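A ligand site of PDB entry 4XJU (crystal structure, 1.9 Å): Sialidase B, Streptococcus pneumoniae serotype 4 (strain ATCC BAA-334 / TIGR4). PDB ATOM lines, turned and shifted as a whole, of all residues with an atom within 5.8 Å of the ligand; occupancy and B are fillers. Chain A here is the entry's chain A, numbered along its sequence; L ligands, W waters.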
ATOM      1  N   ARG A 207      13.216 -15.928  -7.249  1.00  0.00           N
ATOM      2  CA  ARG A 207      12.220 -16.798  -7.844  1.00  0.00           C
ATOM      3  C   ARG A 207      12.395 -18.194  -7.269  1.00  0.00           C
ATOM      4  O   ARG A 207      13.422 -18.496  -6.659  1.00  0.00           O
ATOM      5  CB  ARG A 207      12.366 -16.844  -9.380  1.00  0.00           C
ATOM      6  CG  ARG A 207      11.686 -15.688 -10.164  1.00  0.00           C
ATOM      7  CD  ARG A 207      11.220 -16.153 -11.556  1.00  0.00           C
ATOM      8  NE  ARG A 207      10.278 -17.275 -11.467  1.00  0.00           N
ATOM      9  CZ  ARG A 207       9.893 -18.019 -12.500  1.00  0.00           C
ATOM     10  NH1 ARG A 207      10.334 -17.760 -13.731  1.00  0.00           N
ATOM     11  NH2 ARG A 207       9.036 -19.032 -12.309  1.00  0.00           N
ATOM     12  N   ILE A 208      11.398 -19.041  -7.503  1.00  0.00           N
ATOM     13  CA  ILE A 208      11.473 -20.468  -7.161  1.00  0.00           C
ATOM     14  C   ILE A 208      11.588 -20.728  -5.649  1.00  0.00           C
ATOM     15  O   ILE A 208      12.560 -21.335  -5.182  1.00  0.00           O
ATOM     16  CB  ILE A 208      12.627 -21.183  -7.917  1.00  0.00           C
ATOM     17  CG1 ILE A 208      12.812 -20.628  -9.340  1.00  0.00           C
ATOM     18  CG2 ILE A 208      12.372 -22.671  -7.975  1.00  0.00           C
ATOM     19  CD1 ILE A 208      11.548 -20.715 -10.226  1.00  0.00           C
ATOM     20  N   ASP A 224      15.907 -19.198  -5.436  1.00  0.00           N
ATOM     21  CA  ASP A 224      16.865 -18.689  -6.386  1.00  0.00           C
ATOM     22  C   ASP A 224      17.087 -17.218  -6.048  1.00  0.00           C
ATOM     23  O   ASP A 224      16.151 -16.418  -6.147  1.00  0.00           O
ATOM     24  CB  ASP A 224      16.288 -18.707  -7.813  1.00  0.00           C
ATOM     25  CG  ASP A 224      16.360 -20.069  -8.485  1.00  0.00           C
ATOM     26  OD1 ASP A 224      16.389 -21.137  -7.811  1.00  0.00           O
ATOM     27  OD2 ASP A 224      16.370 -20.064  -9.735  1.00  0.00           O
ATOM     28  N   ARG A 226      18.299 -14.321  -7.784  1.00  0.00           N
ATOM     29  CA  ARG A 226      18.578 -14.021  -9.185  1.00  0.00           C
ATOM     30  C   ARG A 226      19.099 -12.599  -9.366  1.00  0.00           C
ATOM     31  O   ARG A 226      18.407 -11.627  -9.067  1.00  0.00           O
ATOM     32  CB  ARG A 226      17.322 -14.262 -10.051  1.00  0.00           C
ATOM     33  CG  ARG A 226      16.830 -15.726 -10.004  1.00  0.00           C
ATOM     34  CD  ARG A 226      15.920 -16.073 -11.180  1.00  0.00           C
ATOM     35  NE  ARG A 226      15.603 -17.509 -11.180  1.00  0.00           N
ATOM     36  CZ  ARG A 226      14.829 -18.113 -12.086  1.00  0.00           C
ATOM     37  NH1 ARG A 226      14.290 -17.431 -13.089  1.00  0.00           N
ATOM     38  NH2 ARG A 226      14.605 -19.421 -11.983  1.00  0.00           N
ATOM     39  N   ASP A 232      15.784 -16.839 -16.057  1.00  0.00           N
ATOM     40  CA  ASP A 232      16.390 -18.127 -15.728  1.00  0.00           C
ATOM     41  C   ASP A 232      17.788 -18.171 -16.347  1.00  0.00           C
ATOM     42  O   ASP A 232      18.138 -17.322 -17.167  1.00  0.00           O
ATOM     43  CB  ASP A 232      15.549 -19.308 -16.248  1.00  0.00           C
ATOM     44  CG  ASP A 232      15.260 -19.213 -17.741  1.00  0.00           C
ATOM     45  OD1 ASP A 232      14.850 -18.135 -18.214  1.00  0.00           O
ATOM     46  OD2 ASP A 232      15.457 -20.226 -18.451  1.00  0.00           O
ATOM     47  N   SER A 233      18.602 -19.137 -15.930  1.00  0.00           N
ATOM     48  CA  SER A 233      19.928 -19.346 -16.528  1.00  0.00           C
ATOM     49  C   SER A 233      19.791 -19.416 -18.058  1.00  0.00           C
ATOM     50  O   SER A 233      18.779 -19.926 -18.552  1.00  0.00           O
ATOM     51  CB  SER A 233      20.535 -20.649 -16.016  1.00  0.00           C
ATOM     52  OG  SER A 233      20.575 -20.656 -14.591  1.00  0.00           O
ATOM     53  N   ILE A 288      20.142 -23.125 -10.172  1.00  0.00           N
ATOM     54  CA  ILE A 288      18.736 -22.811 -10.438  1.00  0.00           C
ATOM     55  C   ILE A 288      17.857 -23.982 -10.048  1.00  0.00           C
ATOM     56  O   ILE A 288      18.260 -25.124 -10.228  1.00  0.00           O
ATOM     57  CB  ILE A 288      18.537 -22.421 -11.948  1.00  0.00           C
ATOM     58  CG1 ILE A 288      17.072 -22.131 -12.268  1.00  0.00           C
ATOM     59  CG2 ILE A 288      19.093 -23.501 -12.883  1.00  0.00           C
ATOM     60  CD1 ILE A 288      16.920 -21.498 -13.633  1.00  0.00           C
ATOM     61  N   ASP A 289      16.684 -23.686  -9.487  1.00  0.00           N
ATOM     62  CA  ASP A 289      15.680 -24.688  -9.085  1.00  0.00           C
ATOM     63  C   ASP A 289      16.156 -25.610  -7.958  1.00  0.00           C
ATOM     64  O   ASP A 289      16.663 -26.698  -8.230  1.00  0.00           O
ATOM     65  CB  ASP A 289      15.219 -25.522 -10.280  1.00  0.00           C
ATOM     66  CG  ASP A 289      14.450 -24.719 -11.300  1.00  0.00           C
ATOM     67  OD1 ASP A 289      14.107 -23.561 -11.006  1.00  0.00           O
ATOM     68  OD2 ASP A 289      14.207 -25.249 -12.412  1.00  0.00           O
ATOM     69  N   ASP A 306      19.897 -27.466  -9.716  1.00  0.00           N
ATOM     70  CA  ASP A 306      20.610 -27.613 -10.976  1.00  0.00           C
ATOM     71  C   ASP A 306      21.845 -26.737 -10.944  1.00  0.00           C
ATOM     72  O   ASP A 306      21.852 -25.685 -10.285  1.00  0.00           O
ATOM     73  CB  ASP A 306      19.779 -27.167 -12.194  1.00  0.00           C
ATOM     74  CG  ASP A 306      18.424 -27.864 -12.295  1.00  0.00           C
ATOM     75  OD1 ASP A 306      18.241 -29.000 -11.808  1.00  0.00           O
ATOM     76  OD2 ASP A 306      17.510 -27.239 -12.892  1.00  0.00           O
ATOM     77  N   MET A 308      24.579 -24.824 -13.586  1.00  0.00           N
ATOM     78  CA  MET A 308      24.840 -24.408 -14.949  1.00  0.00           C
ATOM     79  C   MET A 308      26.220 -23.782 -15.068  1.00  0.00           C
ATOM     80  O   MET A 308      26.536 -22.836 -14.344  1.00  0.00           O
ATOM     81  CB  MET A 308      23.799 -23.363 -15.377  1.00  0.00           C
ATOM     82  CG  MET A 308      22.368 -23.853 -15.294  1.00  0.00           C
ATOM     83  SD  MET A 308      22.004 -24.999 -16.639  1.00  0.00           S
ATOM     84  CE  MET A 308      20.285 -25.322 -16.248  1.00  0.00           C
ATOM     85  N   ASN A 314      19.020 -23.801 -19.737  1.00  0.00           N
ATOM     86  CA  ASN A 314      18.332 -24.936 -20.360  1.00  0.00           C
ATOM     87  C   ASN A 314      18.302 -24.795 -21.881  1.00  0.00           C
ATOM     88  O   ASN A 314      18.324 -25.789 -22.599  1.00  0.00           O
ATOM     89  CB  ASN A 314      16.939 -25.171 -19.768  1.00  0.00           C
ATOM     90  CG  ASN A 314      15.877 -24.299 -20.410  1.00  0.00           C
ATOM     91  OD1 ASN A 314      15.450 -24.558 -21.536  1.00  0.00           O
ATOM     92  ND2 ASN A 314      15.411 -23.292 -19.674  1.00  0.00           N
ATOM     93  N   TYR A 451      16.228 -32.363 -14.978  1.00  0.00           N
ATOM     94  CA  TYR A 451      15.995 -31.092 -14.310  1.00  0.00           C
ATOM     95  C   TYR A 451      15.296 -31.327 -12.980  1.00  0.00           C
ATOM     96  O   TYR A 451      14.253 -31.992 -12.915  1.00  0.00           O
ATOM     97  CB  TYR A 451      15.173 -30.165 -15.201  1.00  0.00           C
ATOM     98  CG  TYR A 451      15.957 -29.694 -16.402  1.00  0.00           C
ATOM     99  CD1 TYR A 451      16.867 -28.652 -16.281  1.00  0.00           C
ATOM    100  CD2 TYR A 451      15.806 -30.298 -17.643  1.00  0.00           C
ATOM    101  CE1 TYR A 451      17.601 -28.207 -17.365  1.00  0.00           C
ATOM    102  CE2 TYR A 451      16.528 -29.861 -18.745  1.00  0.00           C
ATOM    103  CZ  TYR A 451      17.433 -28.813 -18.592  1.00  0.00           C
ATOM    104  OH  TYR A 451      18.180 -28.351 -19.655  1.00  0.00           O
ATOM    105  N   TYR A 471      12.777 -34.100 -13.947  1.00  0.00           N
ATOM    106  CA  TYR A 471      12.093 -34.362 -15.213  1.00  0.00           C
ATOM    107  C   TYR A 471      13.042 -34.234 -16.406  1.00  0.00           C
ATOM    108  O   TYR A 471      14.042 -33.524 -16.355  1.00  0.00           O
ATOM    109  CB  TYR A 471      10.884 -33.443 -15.393  1.00  0.00           C
ATOM    110  CG  TYR A 471      11.252 -31.971 -15.509  1.00  0.00           C
ATOM    111  CD1 TYR A 471      11.338 -31.172 -14.376  1.00  0.00           C
ATOM    112  CD2 TYR A 471      11.498 -31.389 -16.756  1.00  0.00           C
ATOM    113  CE1 TYR A 471      11.661 -29.823 -14.480  1.00  0.00           C
ATOM    114  CE2 TYR A 471      11.831 -30.039 -16.862  1.00  0.00           C
ATOM    115  CZ  TYR A 471      11.908 -29.262 -15.719  1.00  0.00           C
ATOM    116  OH  TYR A 471      12.245 -27.925 -15.808  1.00  0.00           O
ATOM    117  N   THR A 501       7.844 -29.091 -19.224  1.00  0.00           N
ATOM    118  CA  THR A 501       8.489 -28.694 -17.985  1.00  0.00           C
ATOM    119  C   THR A 501       7.695 -29.384 -16.882  1.00  0.00           C
ATOM    120  O   THR A 501       6.840 -28.781 -16.244  1.00  0.00           O
ATOM    121  CB  THR A 501       8.436 -27.163 -17.816  1.00  0.00           C
ATOM    122  OG1 THR A 501       9.040 -26.559 -18.978  1.00  0.00           O
ATOM    123  CG2 THR A 501       9.191 -26.715 -16.578  1.00  0.00           C
ATOM    124  N   GLU A 503       7.431 -30.235 -13.835  1.00  0.00           N
ATOM    125  CA  GLU A 503       7.754 -30.015 -12.430  1.00  0.00           C
ATOM    126  C   GLU A 503       6.773 -30.778 -11.550  1.00  0.00           C
ATOM    127  O   GLU A 503       5.542 -30.596 -11.649  1.00  0.00           O
ATOM    128  CB  GLU A 503       7.769 -28.514 -12.113  1.00  0.00           C
ATOM    129  CG  GLU A 503       8.875 -27.757 -12.862  1.00  0.00           C
ATOM    130  CD  GLU A 503       8.583 -26.284 -13.038  1.00  0.00           C
ATOM    131  OE1 GLU A 503       9.545 -25.487 -13.193  1.00  0.00           O
ATOM    132  OE2 GLU A 503       7.375 -25.905 -13.022  1.00  0.00           O
ATOM    133  N   ARG A 519       3.159 -30.585 -13.359  1.00  0.00           N
ATOM    134  CA  ARG A 519       2.881 -29.637 -14.446  1.00  0.00           C
ATOM    135  C   ARG A 519       2.942 -30.367 -15.780  1.00  0.00           C
ATOM    136  O   ARG A 519       3.789 -31.249 -15.983  1.00  0.00           O
ATOM    137  CB  ARG A 519       3.954 -28.538 -14.428  1.00  0.00           C
ATOM    138  CG  ARG A 519       3.929 -27.529 -15.570  1.00  0.00           C
ATOM    139  CD  ARG A 519       4.994 -26.473 -15.311  1.00  0.00           C
ATOM    140  NE  ARG A 519       5.266 -25.611 -16.464  1.00  0.00           N
ATOM    141  CZ  ARG A 519       6.132 -24.617 -16.434  1.00  0.00           C
ATOM    142  NH1 ARG A 519       6.812 -24.356 -15.310  1.00  0.00           N
ATOM    143  NH2 ARG A 519       6.338 -23.875 -17.519  1.00  0.00           N
ATOM    144  N   GLY A 552       1.816 -24.161 -18.383  1.00  0.00           N
ATOM    145  CA  GLY A 552       1.708 -24.694 -17.031  1.00  0.00           C
ATOM    146  C   GLY A 552       2.567 -23.952 -16.020  1.00  0.00           C
ATOM    147  O   GLY A 552       3.351 -23.071 -16.369  1.00  0.00           O
ATOM    148  N   ARG A 581      -0.508 -16.747 -15.212  1.00  0.00           N
ATOM    149  CA  ARG A 581      -0.160 -17.186 -13.857  1.00  0.00           C
ATOM    150  C   ARG A 581      -0.799 -16.222 -12.892  1.00  0.00           C
ATOM    151  O   ARG A 581      -0.191 -15.242 -12.470  1.00  0.00           O
ATOM    152  CB  ARG A 581       1.365 -17.236 -13.669  1.00  0.00           C
ATOM    153  CG  ARG A 581       2.005 -18.308 -14.587  1.00  0.00           C
ATOM    154  CD  ARG A 581       3.473 -18.496 -14.347  1.00  0.00           C
ATOM    155  NE  ARG A 581       3.924 -19.765 -14.930  1.00  0.00           N
ATOM    156  CZ  ARG A 581       5.199 -20.088 -15.134  1.00  0.00           C
ATOM    157  NH1 ARG A 581       6.149 -19.234 -14.809  1.00  0.00           N
ATOM    158  NH2 ARG A 581       5.493 -21.266 -15.657  1.00  0.00           N
ATOM    159  N   TYR A 615       4.951 -19.602  -9.172  1.00  0.00           N
ATOM    160  CA  TYR A 615       5.515 -20.718  -8.403  1.00  0.00           C
ATOM    161  C   TYR A 615       5.223 -20.504  -6.922  1.00  0.00           C
ATOM    162  O   TYR A 615       5.081 -19.376  -6.462  1.00  0.00           O
ATOM    163  CB  TYR A 615       7.028 -20.847  -8.603  1.00  0.00           C
ATOM    164  CG  TYR A 615       7.465 -21.476  -9.908  1.00  0.00           C
ATOM    165  CD1 TYR A 615       6.872 -21.139 -11.122  1.00  0.00           C
ATOM    166  CD2 TYR A 615       8.516 -22.389  -9.936  1.00  0.00           C
ATOM    167  CE1 TYR A 615       7.304 -21.711 -12.327  1.00  0.00           C
ATOM    168  CE2 TYR A 615       8.960 -22.952 -11.131  1.00  0.00           C
ATOM    169  CZ  TYR A 615       8.352 -22.610 -12.311  1.00  0.00           C
ATOM    170  OH  TYR A 615       8.813 -23.187 -13.470  1.00  0.00           O
ATOM    171  N   SER A 635       5.087 -14.757 -13.504  1.00  0.00           N
ATOM    172  CA  SER A 635       6.498 -14.960 -13.839  1.00  0.00           C
ATOM    173  C   SER A 635       6.720 -15.496 -15.258  1.00  0.00           C
ATOM    174  O   SER A 635       7.857 -15.773 -15.667  1.00  0.00           O
ATOM    175  CB  SER A 635       7.201 -15.857 -12.810  1.00  0.00           C
ATOM    176  OG  SER A 635       6.558 -17.116 -12.719  1.00  0.00           O
ATOM    177  N   TRP A 636       5.623 -15.650 -16.008  1.00  0.00           N
ATOM    178  CA  TRP A 636       5.719 -16.015 -17.424  1.00  0.00           C
ATOM    179  C   TRP A 636       5.644 -14.753 -18.269  1.00  0.00           C
ATOM    180  O   TRP A 636       6.397 -14.596 -19.240  1.00  0.00           O
ATOM    181  CB  TRP A 636       4.578 -16.974 -17.810  1.00  0.00           C
ATOM    182  CG  TRP A 636       4.747 -17.565 -19.197  1.00  0.00           C
ATOM    183  CD1 TRP A 636       4.216 -17.091 -20.373  1.00  0.00           C
ATOM    184  CD2 TRP A 636       5.498 -18.742 -19.544  1.00  0.00           C
ATOM    185  NE1 TRP A 636       4.601 -17.886 -21.425  1.00  0.00           N
ATOM    186  CE2 TRP A 636       5.397 -18.910 -20.941  1.00  0.00           C
ATOM    187  CE3 TRP A 636       6.262 -19.658 -18.815  1.00  0.00           C
ATOM    188  CZ2 TRP A 636       6.006 -19.963 -21.625  1.00  0.00           C
ATOM    189  CZ3 TRP A 636       6.881 -20.712 -19.492  1.00  0.00           C
ATOM    190  CH2 TRP A 636       6.751 -20.851 -20.879  1.00  0.00           C
HETATM  191  C1  LIG L   1       9.216 -21.044 -15.747  1.00  0.00           C
HETATM  192  O1  LIG L   1       8.391 -21.765 -16.383  1.00  0.00           O
HETATM  193  O2  LIG L   1       8.936 -19.967 -15.219  1.00  0.00           O
HETATM  194  C2  LIG L   1      10.628 -21.575 -15.664  1.00  0.00           C
HETATM  195  C3  LIG L   1      11.403 -21.193 -14.378  1.00  0.00           C
HETATM  196  C4  LIG L   1      12.423 -22.336 -13.979  1.00  0.00           C
HETATM  197  O3  LIG L   1      13.396 -21.766 -13.103  1.00  0.00           O
HETATM  198  C5  LIG L   1      13.118 -22.928 -15.315  1.00  0.00           C
HETATM  199  N1  LIG L   1      14.058 -23.976 -14.941  1.00  0.00           N
HETATM  200  C6  LIG L   1      12.010 -23.257 -16.341  1.00  0.00           C
HETATM  201  O4  LIG L   1      10.697 -22.995 -15.832  1.00  0.00           O
HETATM  202  C7  LIG L   1      12.036 -22.157 -17.400  1.00  0.00           C
HETATM  203  O5  LIG L   1      11.297 -21.052 -16.818  1.00  0.00           O
HETATM  204  C8  LIG L   1      11.553 -22.538 -18.819  1.00  0.00           C
HETATM  205  O6  LIG L   1      10.199 -23.038 -18.883  1.00  0.00           O
HETATM  206  C9  LIG L   1      12.472 -23.573 -19.463  1.00  0.00           C
HETATM  207  O7  LIG L   1      12.228 -24.885 -18.948  1.00  0.00           O
HETATM  208  C10 LIG L   1      15.157 -24.149 -15.678  1.00  0.00           C
HETATM  209  O8  LIG L   1      15.402 -23.451 -16.663  1.00  0.00           O
HETATM  210  C11 LIG L   1      16.070 -25.238 -15.234  1.00  0.00           C
HETATM  211  F1  LIG L   1      11.817 -20.175 -14.491  1.00  0.00           F
HETATM  212  O   HOH W   1      14.014 -20.773 -20.594  1.00  0.00           O
HETATM  213  O   HOH W   2      11.538 -18.464 -17.821  1.00  0.00           O
HETATM  214  O   HOH W   3      17.826 -22.315 -17.583  1.00  0.00           O
HETATM  215  O   HOH W   4       9.116 -17.755 -16.823  1.00  0.00           O
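Water W4 lies within hydrogen-bond range of the backbone carbonyl oxygen (O) of Ser 635 (2.6 Å), an oxygen (O2) of the ligand (2.7 Å) and the guanidinium group (NH1) of Arg 207 (3.3 Å).
Water W2 bridges O5 of the ligand and OD1 of Asp 232.
Water W1 lies within hydrogen-bond range of the side-chain carboxylate of Asp 232 and the side-chain amide nitrogen of Asn 314.
The backbone NH (N) of Asp 289 is in hydrogen-bond range of the side-chain carboxylate (OD1) of Asp 224, 3.1 Å away.
The guanidinium group (NH1) of Arg 581 lies within hydrogen-bond range of the side-chain hydroxyl (OG) of Ser 635 (3.0 Å).
O of Gly 552 is in hydrogen-bond range of NH2 of Arg 581, 2.9 Å away.
The backbone carbonyl oxygen (O) of Arg 207 sits at hydrogen-bond distance from the backbone NH (N) of Asp 224, 2.9 Å away.
ND2 of Asn 314 is in hydrogen-bond range of OD2 of Asp 232, 3.3 Å away.
The guanidinium group of Arg 519 lies within hydrogen-bond range of the side-chain hydroxyl of Tyr 615 (3.0 Å).
The side-chain carboxylate (OE1) of Glu 503 is in hydrogen-bond range of the side-chain hydroxyl (OH) of Tyr 615 (2.4 Å).
O of Tyr 451 sits at hydrogen-bond distance from N of Tyr 471 (2.8 Å).
OD2 of Asp 289 is in hydrogen-bond range of N1 of the ligand, at 2.8 Å.
An oxygen (O3) of the ligand is in hydrogen-bond range of the guanidinium group (NH2) of Arg 226 (2.9 Å).
The guanidinium group (NH1) of Arg 581 is in salt-bridge range of an oxygen (O2) of the ligand.
An oxygen (O2) of the ligand is in salt-bridge range of the guanidinium group (NH1) of Arg 207.
ND2 of Asn 314 sits close to O8 of the ligand (3.0 Å).
The side-chain hydroxyl (OH) of Tyr 615 lies within hydrogen-bond range of an oxygen (O4) of the ligand.
An oxygen (O1) of the ligand lies within salt-bridge range of the guanidinium group (NH2) of Arg 519 (3.2 Å).
Ile 208 touches the ligand.
OD2 of Asp 232 touches O8 of the ligand, at 3.7 Å.
Ile 288 touches the ligand (CD1 to O3, 3.6 Å).
OD2 of Asp 306 touches C11 of the ligand (3.4 Å).
Tyr 451 touches the ligand.
OG1 of Thr 501 touches O7 of the ligand, at 3.6 Å.
Glu 503 touches the ligand (OE1 to O4, 3.8 Å).
Trp 636 touches the ligand.
Hydrophobic or aromatic side chains within 4 Å of the ligand: Ile 208, Ile 288, Tyr 451, Tyr 615 and Trp 636.
15 residues have an atom within 4 Å of the ligand: Arg 207, Ile 208, Arg 226, Asp 232, Ile 288, Asp 289, Asp 306, Asn 314, Tyr 451, Thr 501, Glu 503, Arg 519, Arg 581, Tyr 615 and Trp 636.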
